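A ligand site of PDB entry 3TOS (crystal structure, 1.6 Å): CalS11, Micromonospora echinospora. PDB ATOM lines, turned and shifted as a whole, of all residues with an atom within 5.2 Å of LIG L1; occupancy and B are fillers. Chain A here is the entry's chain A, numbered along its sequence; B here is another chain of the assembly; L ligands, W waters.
N1 of LIG L1 lies within salt-bridge range of OD2 of Asp 189 (2.7 Å).
OD2 of Asp 107 lies within hydrogen-bond range of O4 of LIG L1, 2.7 Å away.
A nitrogen (N1) of LIG L1 is in hydrogen-bond range of the backbone carbonyl oxygen (O) of Gly 77 (2.8 Å).
OE2 of Glu 75 lies within salt-bridge range of N1 of LIG L1 (2.9 Å).
The guanidinium group (NE) of Arg 82 lies within salt-bridge range of an oxygen (O2) of LIG L1.
A nitrogen (N5) of LIG L1 is in hydrogen-bond range of the backbone NH of Val 167 (3.0 Å).
N4 of LIG L1 is in hydrogen-bond range of OD1 of Asp 166, at 3.1 Å.
The backbone carbonyl oxygen (O) of Gly 111 sits close to an oxygen (O5) of LIG L1, at 3.3 Å.
The backbone NH (N) of Thr 108 lies within hydrogen-bond range of a nitrogen (N6) of LIG L1, 3.3 Å away.
O5 of LIG L1 sits at hydrogen-bond distance from OG1 of Thr 108 (3.3 Å).
ND1 of His 83 lies close to O2 of LIG L1 (3.5 Å).
The side-chain carboxylate (OD1) of Asp 189 is in salt-bridge range of a nitrogen (N1) of LG2 L2 (3.6 Å).
O of Asp 107 sits at hydrogen-bond distance from N of Gly 165, at 2.9 Å.
The backbone NH (N) of Val 78 sits at hydrogen-bond distance from the side-chain carboxylate (OD2) of Asp 107, at 2.8 Å.
The backbone carbonyl oxygen of Phe 106 is in hydrogen-bond range of the backbone NH of Gly 77, 2.9 Å away.
A ring nitrogen (ND1) of His 83 sits at hydrogen-bond distance from the side-chain carboxylate (OE2) of Glu 75, at 2.6 Å.
NE2 of His 83 sits at hydrogen-bond distance from NH2 of Arg 82 (3.5 Å).
The backbone NH (N) of Thr 108 sits at hydrogen-bond distance from the backbone carbonyl oxygen (O) of Gly 165, at 3.4 Å.
OG1 of Thr 108 lies within hydrogen-bond range of N of Thr 110 (2.9 Å).
N of Leu 190 sits at hydrogen-bond distance from O of Phe 76, at 3.3 Å.
Val 78 touches LIG L1.
Arg 79 touches LIG L1 (N to O4, 3.6 Å).
Phe 112 touches LIG L1 (CD1 to C10, 3.6 Å).
Pro 113 touches LIG L1.
Phe 130 touches LIG L1.
Gly 165 touches LIG L1 (O to C13, 3.3 Å).
Leu 190 touches LIG L1 (O to C10, 3.3 Å).
Asp 191 touches LIG L1 (OD2 to C5, 3.7 Å).
CD1 of Leu 192 touches N3 of LIG L1 (3.9 Å).
Pro 195 touches LIG L1 (CB to N4, 3.4 Å).
Of the 27 residues printed, 20 come within 4 Å of LIG L1.
The nearest printed residue that does not touch LIG L1 is Arg 168 (4.2 Å).
Water W3 lies within hydrogen-bond range of OD1 of Asn 43 of chain B (2.7 Å), O1 of LIG L1 (2.8 Å), N of Arg 82 (3.2 Å) and O of Val 78 (3.5 Å).
Water W1 lies within hydrogen-bond range of O1 of LIG L1 (2.9 Å) and NH1 of Arg 79 (3.0 Å).
Water W6 bridges N4 of LIG L1 (3.0 Å) and NH2 of Arg 168 (3.4 Å).
Water W5 lies within hydrogen-bond range of O of Phe 130 (2.9 Å), N of Gly 111 (3.1 Å), O4 of LIG L1 (3.1 Å), OD1 of Asp 107 (3.3 Å) and N of Thr 110 (3.5 Å).
Water W7 lies within hydrogen-bond range of OE1 of Glu 75 (2.5 Å), O of Val 78 (2.9 Å), N of His 83 (2.9 Å), N of Arg 82 (3.3 Å) and N1 of LIG L1 (3.4 Å).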
ATOM      1  N   GLU A  75       6.624 -26.144  18.518  1.00  0.00           N
ATOM      2  CA  GLU A  75       5.614 -25.214  19.040  1.00  0.00           C
ATOM      3  C   GLU A  75       6.024 -24.820  20.421  1.00  0.00           C
ATOM      4  O   GLU A  75       6.294 -25.690  21.275  1.00  0.00           O
ATOM      5  CB  GLU A  75       4.231 -25.855  19.070  1.00  0.00           C
ATOM      6  CG  GLU A  75       3.208 -24.815  19.600  1.00  0.00           C
ATOM      7  CD  GLU A  75       1.728 -25.267  19.566  1.00  0.00           C
ATOM      8  OE1 GLU A  75       1.401 -26.397  20.013  1.00  0.00           O
ATOM      9  OE2 GLU A  75       0.876 -24.420  19.189  1.00  0.00           O
ATOM     10  N   PHE A  76       6.047 -23.508  20.670  1.00  0.00           N
ATOM     11  CA  PHE A  76       6.278 -22.973  21.989  1.00  0.00           C
ATOM     12  C   PHE A  76       4.942 -22.482  22.558  1.00  0.00           C
ATOM     13  O   PHE A  76       4.387 -21.468  22.109  1.00  0.00           O
ATOM     14  CB  PHE A  76       7.284 -21.832  21.872  1.00  0.00           C
ATOM     15  CG  PHE A  76       8.485 -22.193  21.036  1.00  0.00           C
ATOM     16  CD1 PHE A  76       9.412 -23.133  21.477  1.00  0.00           C
ATOM     17  CD2 PHE A  76       8.677 -21.565  19.822  1.00  0.00           C
ATOM     18  CE1 PHE A  76      10.518 -23.453  20.686  1.00  0.00           C
ATOM     19  CE2 PHE A  76       9.747 -21.893  19.048  1.00  0.00           C
ATOM     20  CZ  PHE A  76      10.678 -22.847  19.457  1.00  0.00           C
ATOM     21  N   GLY A  77       4.388 -23.275  23.493  1.00  0.00           N
ATOM     22  CA  GLY A  77       3.059 -23.026  24.079  1.00  0.00           C
ATOM     23  C   GLY A  77       2.073 -24.008  23.439  1.00  0.00           C
ATOM     24  O   GLY A  77       1.507 -23.719  22.348  1.00  0.00           O
ATOM     25  N   VAL A  78       1.847 -25.126  24.143  1.00  0.00           N
ATOM     26  CA  VAL A  78       1.103 -26.303  23.629  1.00  0.00           C
ATOM     27  C   VAL A  78      -0.285 -26.381  24.201  1.00  0.00           C
ATOM     28  O   VAL A  78      -1.218 -26.763  23.506  1.00  0.00           O
ATOM     29  CB  VAL A  78       1.919 -27.551  24.053  1.00  0.00           C
ATOM     30  CG1 VAL A  78       1.166 -28.816  23.778  1.00  0.00           C
ATOM     31  CG2 VAL A  78       3.279 -27.546  23.260  1.00  0.00           C
ATOM     32  N   ARG A  79      -0.415 -26.045  25.477  1.00  0.00           N
ATOM     33  CA  ARG A  79      -1.679 -26.232  26.211  1.00  0.00           C
ATOM     34  C   ARG A  79      -2.170 -27.673  26.051  1.00  0.00           C
ATOM     35  O   ARG A  79      -1.440 -28.610  26.461  1.00  0.00           O
ATOM     36  CB  ARG A  79      -2.742 -25.132  25.897  1.00  0.00           C
ATOM     37  CG  ARG A  79      -3.926 -25.042  26.896  1.00  0.00           C
ATOM     38  CD  ARG A  79      -5.014 -24.181  26.295  1.00  0.00           C
ATOM     39  NE  ARG A  79      -6.047 -23.885  27.297  1.00  0.00           N
ATOM     40  CZ  ARG A  79      -7.135 -23.108  27.126  1.00  0.00           C
ATOM     41  NH1 ARG A  79      -7.409 -22.507  25.956  1.00  0.00           N
ATOM     42  NH2 ARG A  79      -7.983 -22.936  28.177  1.00  0.00           N
ATOM     43  N   ARG A  82      -3.681 -28.965  20.714  1.00  0.00           N
ATOM     44  CA  ARG A  82      -4.403 -28.769  19.432  1.00  0.00           C
ATOM     45  C   ARG A  82      -3.504 -28.764  18.197  1.00  0.00           C
ATOM     46  O   ARG A  82      -3.788 -29.482  17.209  1.00  0.00           O
ATOM     47  CB  ARG A  82      -5.132 -27.426  19.455  1.00  0.00           C
ATOM     48  CG  ARG A  82      -5.817 -27.126  18.121  1.00  0.00           C
ATOM     49  CD  ARG A  82      -6.589 -25.814  18.183  1.00  0.00           C
ATOM     50  NE  ARG A  82      -5.784 -24.639  18.523  1.00  0.00           N
ATOM     51  CZ  ARG A  82      -6.191 -23.386  18.353  1.00  0.00           C
ATOM     52  NH1 ARG A  82      -7.382 -23.124  17.805  1.00  0.00           N
ATOM     53  NH2 ARG A  82      -5.383 -22.374  18.688  1.00  0.00           N
ATOM     54  N   HIS A  83      -2.460 -27.945  18.225  1.00  0.00           N
ATOM     55  CA  HIS A  83      -1.599 -27.851  17.066  1.00  0.00           C
ATOM     56  C   HIS A  83      -0.731 -29.070  16.889  1.00  0.00           C
ATOM     57  O   HIS A  83      -0.444 -29.458  15.728  1.00  0.00           O
ATOM     58  CB  HIS A  83      -0.713 -26.593  17.096  1.00  0.00           C
ATOM     59  CG  HIS A  83      -1.511 -25.327  16.965  1.00  0.00           C
ATOM     60  ND1 HIS A  83      -1.093 -24.120  17.495  1.00  0.00           N
ATOM     61  CD2 HIS A  83      -2.732 -25.093  16.387  1.00  0.00           C
ATOM     62  CE1 HIS A  83      -2.001 -23.188  17.226  1.00  0.00           C
ATOM     63  NE2 HIS A  83      -3.010 -23.757  16.555  1.00  0.00           N
ATOM     64  N   PHE A 106       6.852 -27.461  23.512  1.00  0.00           N
ATOM     65  CA  PHE A 106       7.397 -26.941  24.789  1.00  0.00           C
ATOM     66  C   PHE A 106       6.309 -26.264  25.600  1.00  0.00           C
ATOM     67  O   PHE A 106       5.596 -25.380  25.087  1.00  0.00           O
ATOM     68  CB  PHE A 106       8.491 -25.896  24.535  1.00  0.00           C
ATOM     69  CG  PHE A 106       9.732 -26.435  23.827  1.00  0.00           C
ATOM     70  CD1 PHE A 106       9.767 -26.535  22.410  1.00  0.00           C
ATOM     71  CD2 PHE A 106      10.862 -26.776  24.559  1.00  0.00           C
ATOM     72  CE1 PHE A 106      10.888 -26.978  21.744  1.00  0.00           C
ATOM     73  CE2 PHE A 106      12.032 -27.220  23.895  1.00  0.00           C
ATOM     74  CZ  PHE A 106      12.009 -27.399  22.496  1.00  0.00           C
ATOM     75  N   ASP A 107       6.186 -26.631  26.870  1.00  0.00           N
ATOM     76  CA  ASP A 107       5.274 -25.904  27.730  1.00  0.00           C
ATOM     77  C   ASP A 107       5.648 -26.229  29.188  1.00  0.00           C
ATOM     78  O   ASP A 107       6.279 -27.260  29.466  1.00  0.00           O
ATOM     79  CB  ASP A 107       3.830 -26.395  27.451  1.00  0.00           C
ATOM     80  CG  ASP A 107       2.771 -25.366  27.796  1.00  0.00           C
ATOM     81  OD1 ASP A 107       2.682 -24.884  28.952  1.00  0.00           O
ATOM     82  OD2 ASP A 107       1.995 -24.976  26.911  1.00  0.00           O
ATOM     83  N   THR A 108       5.231 -25.359  30.109  1.00  0.00           N
ATOM     84  CA  THR A 108       5.317 -25.744  31.506  1.00  0.00           C
ATOM     85  C   THR A 108       4.250 -26.835  31.816  1.00  0.00           C
ATOM     86  O   THR A 108       4.393 -27.653  32.742  1.00  0.00           O
ATOM     87  CB  THR A 108       4.946 -24.562  32.432  1.00  0.00           C
ATOM     88  OG1 THR A 108       3.627 -24.151  32.086  1.00  0.00           O
ATOM     89  CG2 THR A 108       5.969 -23.388  32.335  1.00  0.00           C
ATOM     90  N   PHE A 109       3.150 -26.761  31.063  1.00  0.00           N
ATOM     91  CA  PHE A 109       1.935 -27.538  31.253  1.00  0.00           C
ATOM     92  C   PHE A 109       1.239 -27.152  32.571  1.00  0.00           C
ATOM     93  O   PHE A 109       0.279 -27.793  33.006  1.00  0.00           O
ATOM     94  CB  PHE A 109       2.148 -29.067  31.082  1.00  0.00           C
ATOM     95  CG  PHE A 109       2.521 -29.430  29.694  1.00  0.00           C
ATOM     96  CD1 PHE A 109       1.550 -29.479  28.697  1.00  0.00           C
ATOM     97  CD2 PHE A 109       3.844 -29.634  29.393  1.00  0.00           C
ATOM     98  CE1 PHE A 109       1.924 -29.784  27.380  1.00  0.00           C
ATOM     99  CE2 PHE A 109       4.224 -29.938  28.088  1.00  0.00           C
ATOM    100  CZ  PHE A 109       3.261 -30.035  27.062  1.00  0.00           C
ATOM    101  N   THR A 110       1.705 -26.053  33.154  1.00  0.00           N
ATOM    102  CA  THR A 110       1.127 -25.567  34.408  1.00  0.00           C
ATOM    103  C   THR A 110       0.769 -24.095  34.246  1.00  0.00           C
ATOM    104  O   THR A 110       0.576 -23.387  35.219  1.00  0.00           O
ATOM    105  CB  THR A 110       2.068 -25.732  35.613  1.00  0.00           C
ATOM    106  OG1 THR A 110       3.263 -24.996  35.375  1.00  0.00           O
ATOM    107  CG2 THR A 110       2.367 -27.214  35.873  1.00  0.00           C
ATOM    108  N   GLY A 111       0.677 -23.665  32.993  1.00  0.00           N
ATOM    109  CA  GLY A 111       0.259 -22.301  32.691  1.00  0.00           C
ATOM    110  C   GLY A 111       1.399 -21.300  32.787  1.00  0.00           C
ATOM    111  O   GLY A 111       2.578 -21.664  33.003  1.00  0.00           O
ATOM    112  N   PHE A 112       1.055 -20.036  32.628  1.00  0.00           N
ATOM    113  CA  PHE A 112       2.112 -19.037  32.567  1.00  0.00           C
ATOM    114  C   PHE A 112       2.940 -19.110  33.881  1.00  0.00           C
ATOM    115  O   PHE A 112       2.383 -19.112  34.981  1.00  0.00           O
ATOM    116  CB  PHE A 112       1.526 -17.601  32.571  1.00  0.00           C
ATOM    117  CG  PHE A 112       0.814 -17.209  31.339  1.00  0.00           C
ATOM    118  CD1 PHE A 112       1.119 -17.748  30.087  1.00  0.00           C
ATOM    119  CD2 PHE A 112      -0.204 -16.270  31.444  1.00  0.00           C
ATOM    120  CE1 PHE A 112       0.422 -17.316  28.960  1.00  0.00           C
ATOM    121  CE2 PHE A 112      -0.885 -15.839  30.294  1.00  0.00           C
ATOM    122  CZ  PHE A 112      -0.591 -16.371  29.070  1.00  0.00           C
ATOM    123  N   PRO A 113       4.276 -19.174  33.806  1.00  0.00           N
ATOM    124  CA  PRO A 113       5.041 -19.355  35.076  1.00  0.00           C
ATOM    125  C   PRO A 113       5.367 -18.035  35.835  1.00  0.00           C
ATOM    126  O   PRO A 113       5.655 -18.000  37.087  1.00  0.00           O
ATOM    127  CB  PRO A 113       6.302 -20.131  34.612  1.00  0.00           C
ATOM    128  CG  PRO A 113       6.450 -19.768  33.176  1.00  0.00           C
ATOM    129  CD  PRO A 113       5.065 -19.462  32.600  1.00  0.00           C
ATOM    130  N   ARG A 129      -2.346 -19.162  34.347  1.00  0.00           N
ATOM    131  CA  ARG A 129      -3.371 -19.110  33.292  1.00  0.00           C
ATOM    132  C   ARG A 129      -2.986 -20.134  32.218  1.00  0.00           C
ATOM    133  O   ARG A 129      -1.801 -20.236  31.832  1.00  0.00           O
ATOM    134  CB  ARG A 129      -3.428 -17.702  32.694  1.00  0.00           C
ATOM    135  CG  ARG A 129      -4.457 -17.517  31.556  1.00  0.00           C
ATOM    136  CD  ARG A 129      -5.842 -17.483  32.138  1.00  0.00           C
ATOM    137  NE  ARG A 129      -6.873 -17.571  31.079  1.00  0.00           N
ATOM    138  CZ  ARG A 129      -8.189 -17.452  31.317  1.00  0.00           C
ATOM    139  NH1 ARG A 129      -8.637 -17.210  32.581  1.00  0.00           N
ATOM    140  NH2 ARG A 129      -9.064 -17.570  30.294  1.00  0.00           N
ATOM    141  N   PHE A 130      -3.992 -20.884  31.753  1.00  0.00           N
ATOM    142  CA  PHE A 130      -3.852 -21.944  30.728  1.00  0.00           C
ATOM    143  C   PHE A 130      -3.261 -23.220  31.277  1.00  0.00           C
ATOM    144  O   PHE A 130      -2.918 -24.122  30.486  1.00  0.00           O
ATOM    145  CB  PHE A 130      -2.999 -21.526  29.473  1.00  0.00           C
ATOM    146  CG  PHE A 130      -3.575 -20.383  28.691  1.00  0.00           C
ATOM    147  CD1 PHE A 130      -4.755 -20.531  28.023  1.00  0.00           C
ATOM    148  CD2 PHE A 130      -2.899 -19.188  28.604  1.00  0.00           C
ATOM    149  CE1 PHE A 130      -5.290 -19.512  27.308  1.00  0.00           C
ATOM    150  CE2 PHE A 130      -3.437 -18.146  27.903  1.00  0.00           C
ATOM    151  CZ  PHE A 130      -4.637 -18.301  27.229  1.00  0.00           C
ATOM    152  N   GLY A 165       8.620 -27.605  31.056  1.00  0.00           N
ATOM    153  CA  GLY A 165       9.281 -26.659  31.906  1.00  0.00           C
ATOM    154  C   GLY A 165       9.275 -25.290  31.275  1.00  0.00           C
ATOM    155  O   GLY A 165       8.576 -25.074  30.298  1.00  0.00           O
ATOM    156  N   ASP A 166      10.026 -24.327  31.857  1.00  0.00           N
ATOM    157  CA  ASP A 166      10.020 -22.953  31.357  1.00  0.00           C
ATOM    158  C   ASP A 166      10.959 -22.932  30.134  1.00  0.00           C
ATOM    159  O   ASP A 166      12.143 -23.327  30.250  1.00  0.00           O
ATOM    160  CB  ASP A 166      10.567 -22.079  32.475  1.00  0.00           C
ATOM    161  CG  ASP A 166      10.494 -20.597  32.179  1.00  0.00           C
ATOM    162  OD1 ASP A 166      10.608 -20.165  31.006  1.00  0.00           O
ATOM    163  OD2 ASP A 166      10.324 -19.834  33.151  1.00  0.00           O
ATOM    164  N   VAL A 167      10.437 -22.457  28.995  1.00  0.00           N
ATOM    165  CA  VAL A 167      11.221 -22.429  27.746  1.00  0.00           C
ATOM    166  C   VAL A 167      12.521 -21.615  27.864  1.00  0.00           C
ATOM    167  O   VAL A 167      13.463 -21.857  27.066  1.00  0.00           O
ATOM    168  CB  VAL A 167      10.402 -21.862  26.556  1.00  0.00           C
ATOM    169  CG1 VAL A 167       9.226 -22.774  26.232  1.00  0.00           C
ATOM    170  CG2 VAL A 167       9.896 -20.401  26.802  1.00  0.00           C
ATOM    171  N   ARG A 168      12.600 -20.669  28.806  1.00  0.00           N
ATOM    172  CA  ARG A 168      13.857 -19.923  28.998  1.00  0.00           C
ATOM    173  C   ARG A 168      15.022 -20.870  29.280  1.00  0.00           C
ATOM    174  O   ARG A 168      16.168 -20.580  28.897  1.00  0.00           O
ATOM    175  CB  ARG A 168      13.745 -18.926  30.150  1.00  0.00           C
ATOM    176  CG  ARG A 168      12.804 -17.758  29.976  1.00  0.00           C
ATOM    177  CD  ARG A 168      12.898 -17.012  31.324  1.00  0.00           C
ATOM    178  NE  ARG A 168      11.998 -15.885  31.549  1.00  0.00           N
ATOM    179  CZ  ARG A 168      10.814 -15.958  32.156  1.00  0.00           C
ATOM    180  NH1 ARG A 168      10.109 -14.865  32.323  1.00  0.00           N
ATOM    181  NH2 ARG A 168      10.307 -17.113  32.568  1.00  0.00           N
ATOM    182  N   ASP A 189       3.492 -19.502  20.385  1.00  0.00           N
ATOM    183  CA  ASP A 189       2.163 -19.333  20.980  1.00  0.00           C
ATOM    184  C   ASP A 189       2.272 -19.287  22.512  1.00  0.00           C
ATOM    185  O   ASP A 189       1.464 -19.898  23.242  1.00  0.00           O
ATOM    186  CB  ASP A 189       1.276 -20.453  20.554  1.00  0.00           C
ATOM    187  CG  ASP A 189      -0.206 -20.131  20.756  1.00  0.00           C
ATOM    188  OD1 ASP A 189      -0.502 -18.957  21.106  1.00  0.00           O
ATOM    189  OD2 ASP A 189      -1.076 -21.049  20.523  1.00  0.00           O
ATOM    190  N   LEU A 190       3.258 -18.498  22.988  1.00  0.00           N
ATOM    191  CA  LEU A 190       3.523 -18.314  24.458  1.00  0.00           C
ATOM    192  C   LEU A 190       2.787 -17.154  25.073  1.00  0.00           C
ATOM    193  O   LEU A 190       2.675 -17.077  26.287  1.00  0.00           O
ATOM    194  CB  LEU A 190       5.035 -18.127  24.719  1.00  0.00           C
ATOM    195  CG  LEU A 190       5.906 -19.265  24.229  1.00  0.00           C
ATOM    196  CD1 LEU A 190       7.357 -18.755  24.075  1.00  0.00           C
ATOM    197  CD2 LEU A 190       5.877 -20.393  25.251  1.00  0.00           C
ATOM    198  N   ASP A 191       2.355 -16.219  24.206  1.00  0.00           N
ATOM    199  CA  ASP A 191       1.697 -14.943  24.580  1.00  0.00           C
ATOM    200  C   ASP A 191       2.626 -13.901  25.230  1.00  0.00           C
ATOM    201  O   ASP A 191       2.509 -12.723  24.957  1.00  0.00           O
ATOM    202  CB  ASP A 191       0.463 -15.168  25.467  1.00  0.00           C
ATOM    203  CG  ASP A 191      -0.600 -15.980  24.786  1.00  0.00           C
ATOM    204  OD1 ASP A 191      -0.898 -15.676  23.647  1.00  0.00           O
ATOM    205  OD2 ASP A 191      -1.041 -16.991  25.324  1.00  0.00           O
ATOM    206  N   LEU A 192       3.523 -14.350  26.108  1.00  0.00           N
ATOM    207  CA  LEU A 192       4.294 -13.452  26.969  1.00  0.00           C
ATOM    208  C   LEU A 192       5.594 -12.961  26.363  1.00  0.00           C
ATOM    209  O   LEU A 192       6.311 -13.683  25.651  1.00  0.00           O
ATOM    210  CB  LEU A 192       4.603 -14.190  28.279  1.00  0.00           C
ATOM    211  CG  LEU A 192       3.413 -14.777  29.018  1.00  0.00           C
ATOM    212  CD1 LEU A 192       3.838 -15.532  30.264  1.00  0.00           C
ATOM    213  CD2 LEU A 192       2.309 -13.761  29.331  1.00  0.00           C
ATOM    214  N   PRO A 195       9.506 -14.939  27.601  1.00  0.00           N
ATOM    215  CA  PRO A 195       9.923 -16.203  26.991  1.00  0.00           C
ATOM    216  C   PRO A 195       9.926 -16.130  25.443  1.00  0.00           C
ATOM    217  O   PRO A 195      10.757 -16.821  24.848  1.00  0.00           O
ATOM    218  CB  PRO A 195       8.830 -17.197  27.463  1.00  0.00           C
ATOM    219  CG  PRO A 195       7.623 -16.333  27.738  1.00  0.00           C
ATOM    220  CD  PRO A 195       8.215 -15.055  28.307  1.00  0.00           C
ATOM    221  N   ASN B  43     -10.162 -29.010  20.570  1.00  0.00           N
ATOM    222  CA  ASN B  43      -8.965 -29.820  20.481  1.00  0.00           C
ATOM    223  C   ASN B  43      -9.185 -31.088  19.676  1.00  0.00           C
ATOM    224  O   ASN B  43      -8.460 -32.052  19.812  1.00  0.00           O
ATOM    225  CB  ASN B  43      -8.442 -30.153  21.882  1.00  0.00           C
ATOM    226  CG  ASN B  43      -7.890 -28.945  22.570  1.00  0.00           C
ATOM    227  OD1 ASN B  43      -6.754 -28.525  22.301  1.00  0.00           O
ATOM    228  ND2 ASN B  43      -8.690 -28.336  23.433  1.00  0.00           N
HETATM  229  N1  LIG L   1      -1.044 -23.635  21.177  1.00  0.00           N
HETATM  230  C1  LIG L   1      -2.227 -23.851  22.118  1.00  0.00           C
HETATM  231  C2  LIG L   1      -2.414 -22.614  23.003  1.00  0.00           C
HETATM  232  C3  LIG L   1      -1.204 -22.289  23.909  1.00  0.00           C
HETATM  233  S1  LIG L   1      -1.719 -21.298  25.310  1.00  0.00           S
HETATM  234  C4  LIG L   1      -3.460 -24.114  21.308  1.00  0.00           C
HETATM  235  O1  LIG L   1      -4.552 -24.372  21.818  1.00  0.00           O
HETATM  236  O2  LIG L   1      -3.381 -24.137  20.080  1.00  0.00           O
HETATM  237  C5  LIG L   1      -0.190 -20.549  25.832  1.00  0.00           C
HETATM  238  C6  LIG L   1       0.774 -21.542  26.510  1.00  0.00           C
HETATM  239  O3  LIG L   1       2.051 -20.928  26.623  1.00  0.00           O
HETATM  240  C7  LIG L   1       0.321 -21.970  27.917  1.00  0.00           C
HETATM  241  O4  LIG L   1       0.057 -23.386  27.888  1.00  0.00           O
HETATM  242  C8  LIG L   1       1.542 -21.598  28.735  1.00  0.00           C
HETATM  243  O5  LIG L   1       1.801 -22.452  29.879  1.00  0.00           O
HETATM  244  C9  LIG L   1       2.701 -21.569  27.725  1.00  0.00           C
HETATM  245  N2  LIG L   1       3.791 -20.736  28.197  1.00  0.00           N
HETATM  246  C10 LIG L   1       3.775 -19.381  28.364  1.00  0.00           C
HETATM  247  N3  LIG L   1       4.976 -18.972  28.853  1.00  0.00           N
HETATM  248  C11 LIG L   1       5.763 -20.075  29.000  1.00  0.00           C
HETATM  249  C12 LIG L   1       7.107 -20.347  29.467  1.00  0.00           C
HETATM  250  N4  LIG L   1       7.888 -19.312  29.896  1.00  0.00           N
HETATM  251  N5  LIG L   1       7.545 -21.629  29.362  1.00  0.00           N
HETATM  252  C13 LIG L   1       6.777 -22.673  28.952  1.00  0.00           C
HETATM  253  N6  LIG L   1       5.508 -22.489  28.540  1.00  0.00           N
HETATM  254  C14 LIG L   1       4.982 -21.228  28.547  1.00  0.00           C
HETATM  255  N1  LG2 L   2      -3.845 -17.595  21.391  1.00  0.00           N
HETATM  256  C1  LG2 L   2      -5.005 -18.394  21.909  1.00  0.00           C
HETATM  257  C2  LG2 L   2      -6.187 -18.366  20.880  1.00  0.00           C
HETATM  258  O1  LG2 L   2      -7.250 -18.965  21.091  1.00  0.00           O
HETATM  259  C3  LG2 L   2      -5.451 -17.875  23.295  1.00  0.00           C
HETATM  260  C4  LG2 L   2      -6.057 -16.415  23.267  1.00  0.00           C
HETATM  261  C5  LG2 L   2      -6.553 -15.948  24.642  1.00  0.00           C
HETATM  262  O2  LG2 L   2      -7.005 -16.787  25.459  1.00  0.00           O
HETATM  263  O3  LG2 L   2      -6.474 -14.734  24.916  1.00  0.00           O
HETATM  264  O4  LG2 L   2      -6.115 -17.745  19.797  1.00  0.00           O
HETATM  265  O   HOH W   1      -5.810 -22.364  23.419  1.00  0.00           O
HETATM  266  O   HOH W   2      -2.011 -18.507  23.387  1.00  0.00           O
HETATM  267  O   HOH W   3      -4.668 -26.923  23.038  1.00  0.00           O
HETATM  268  O   HOH W   4      -7.390 -25.002  21.617  1.00  0.00           O
HETATM  269  O   HOH W   5      -0.229 -25.106  30.437  1.00  0.00           O
HETATM  270  O   HOH W   6       7.223 -16.731  31.215  1.00  0.00           O
HETATM  271  O   HOH W   7      -0.985 -27.000  20.596  1.00  0.00           O
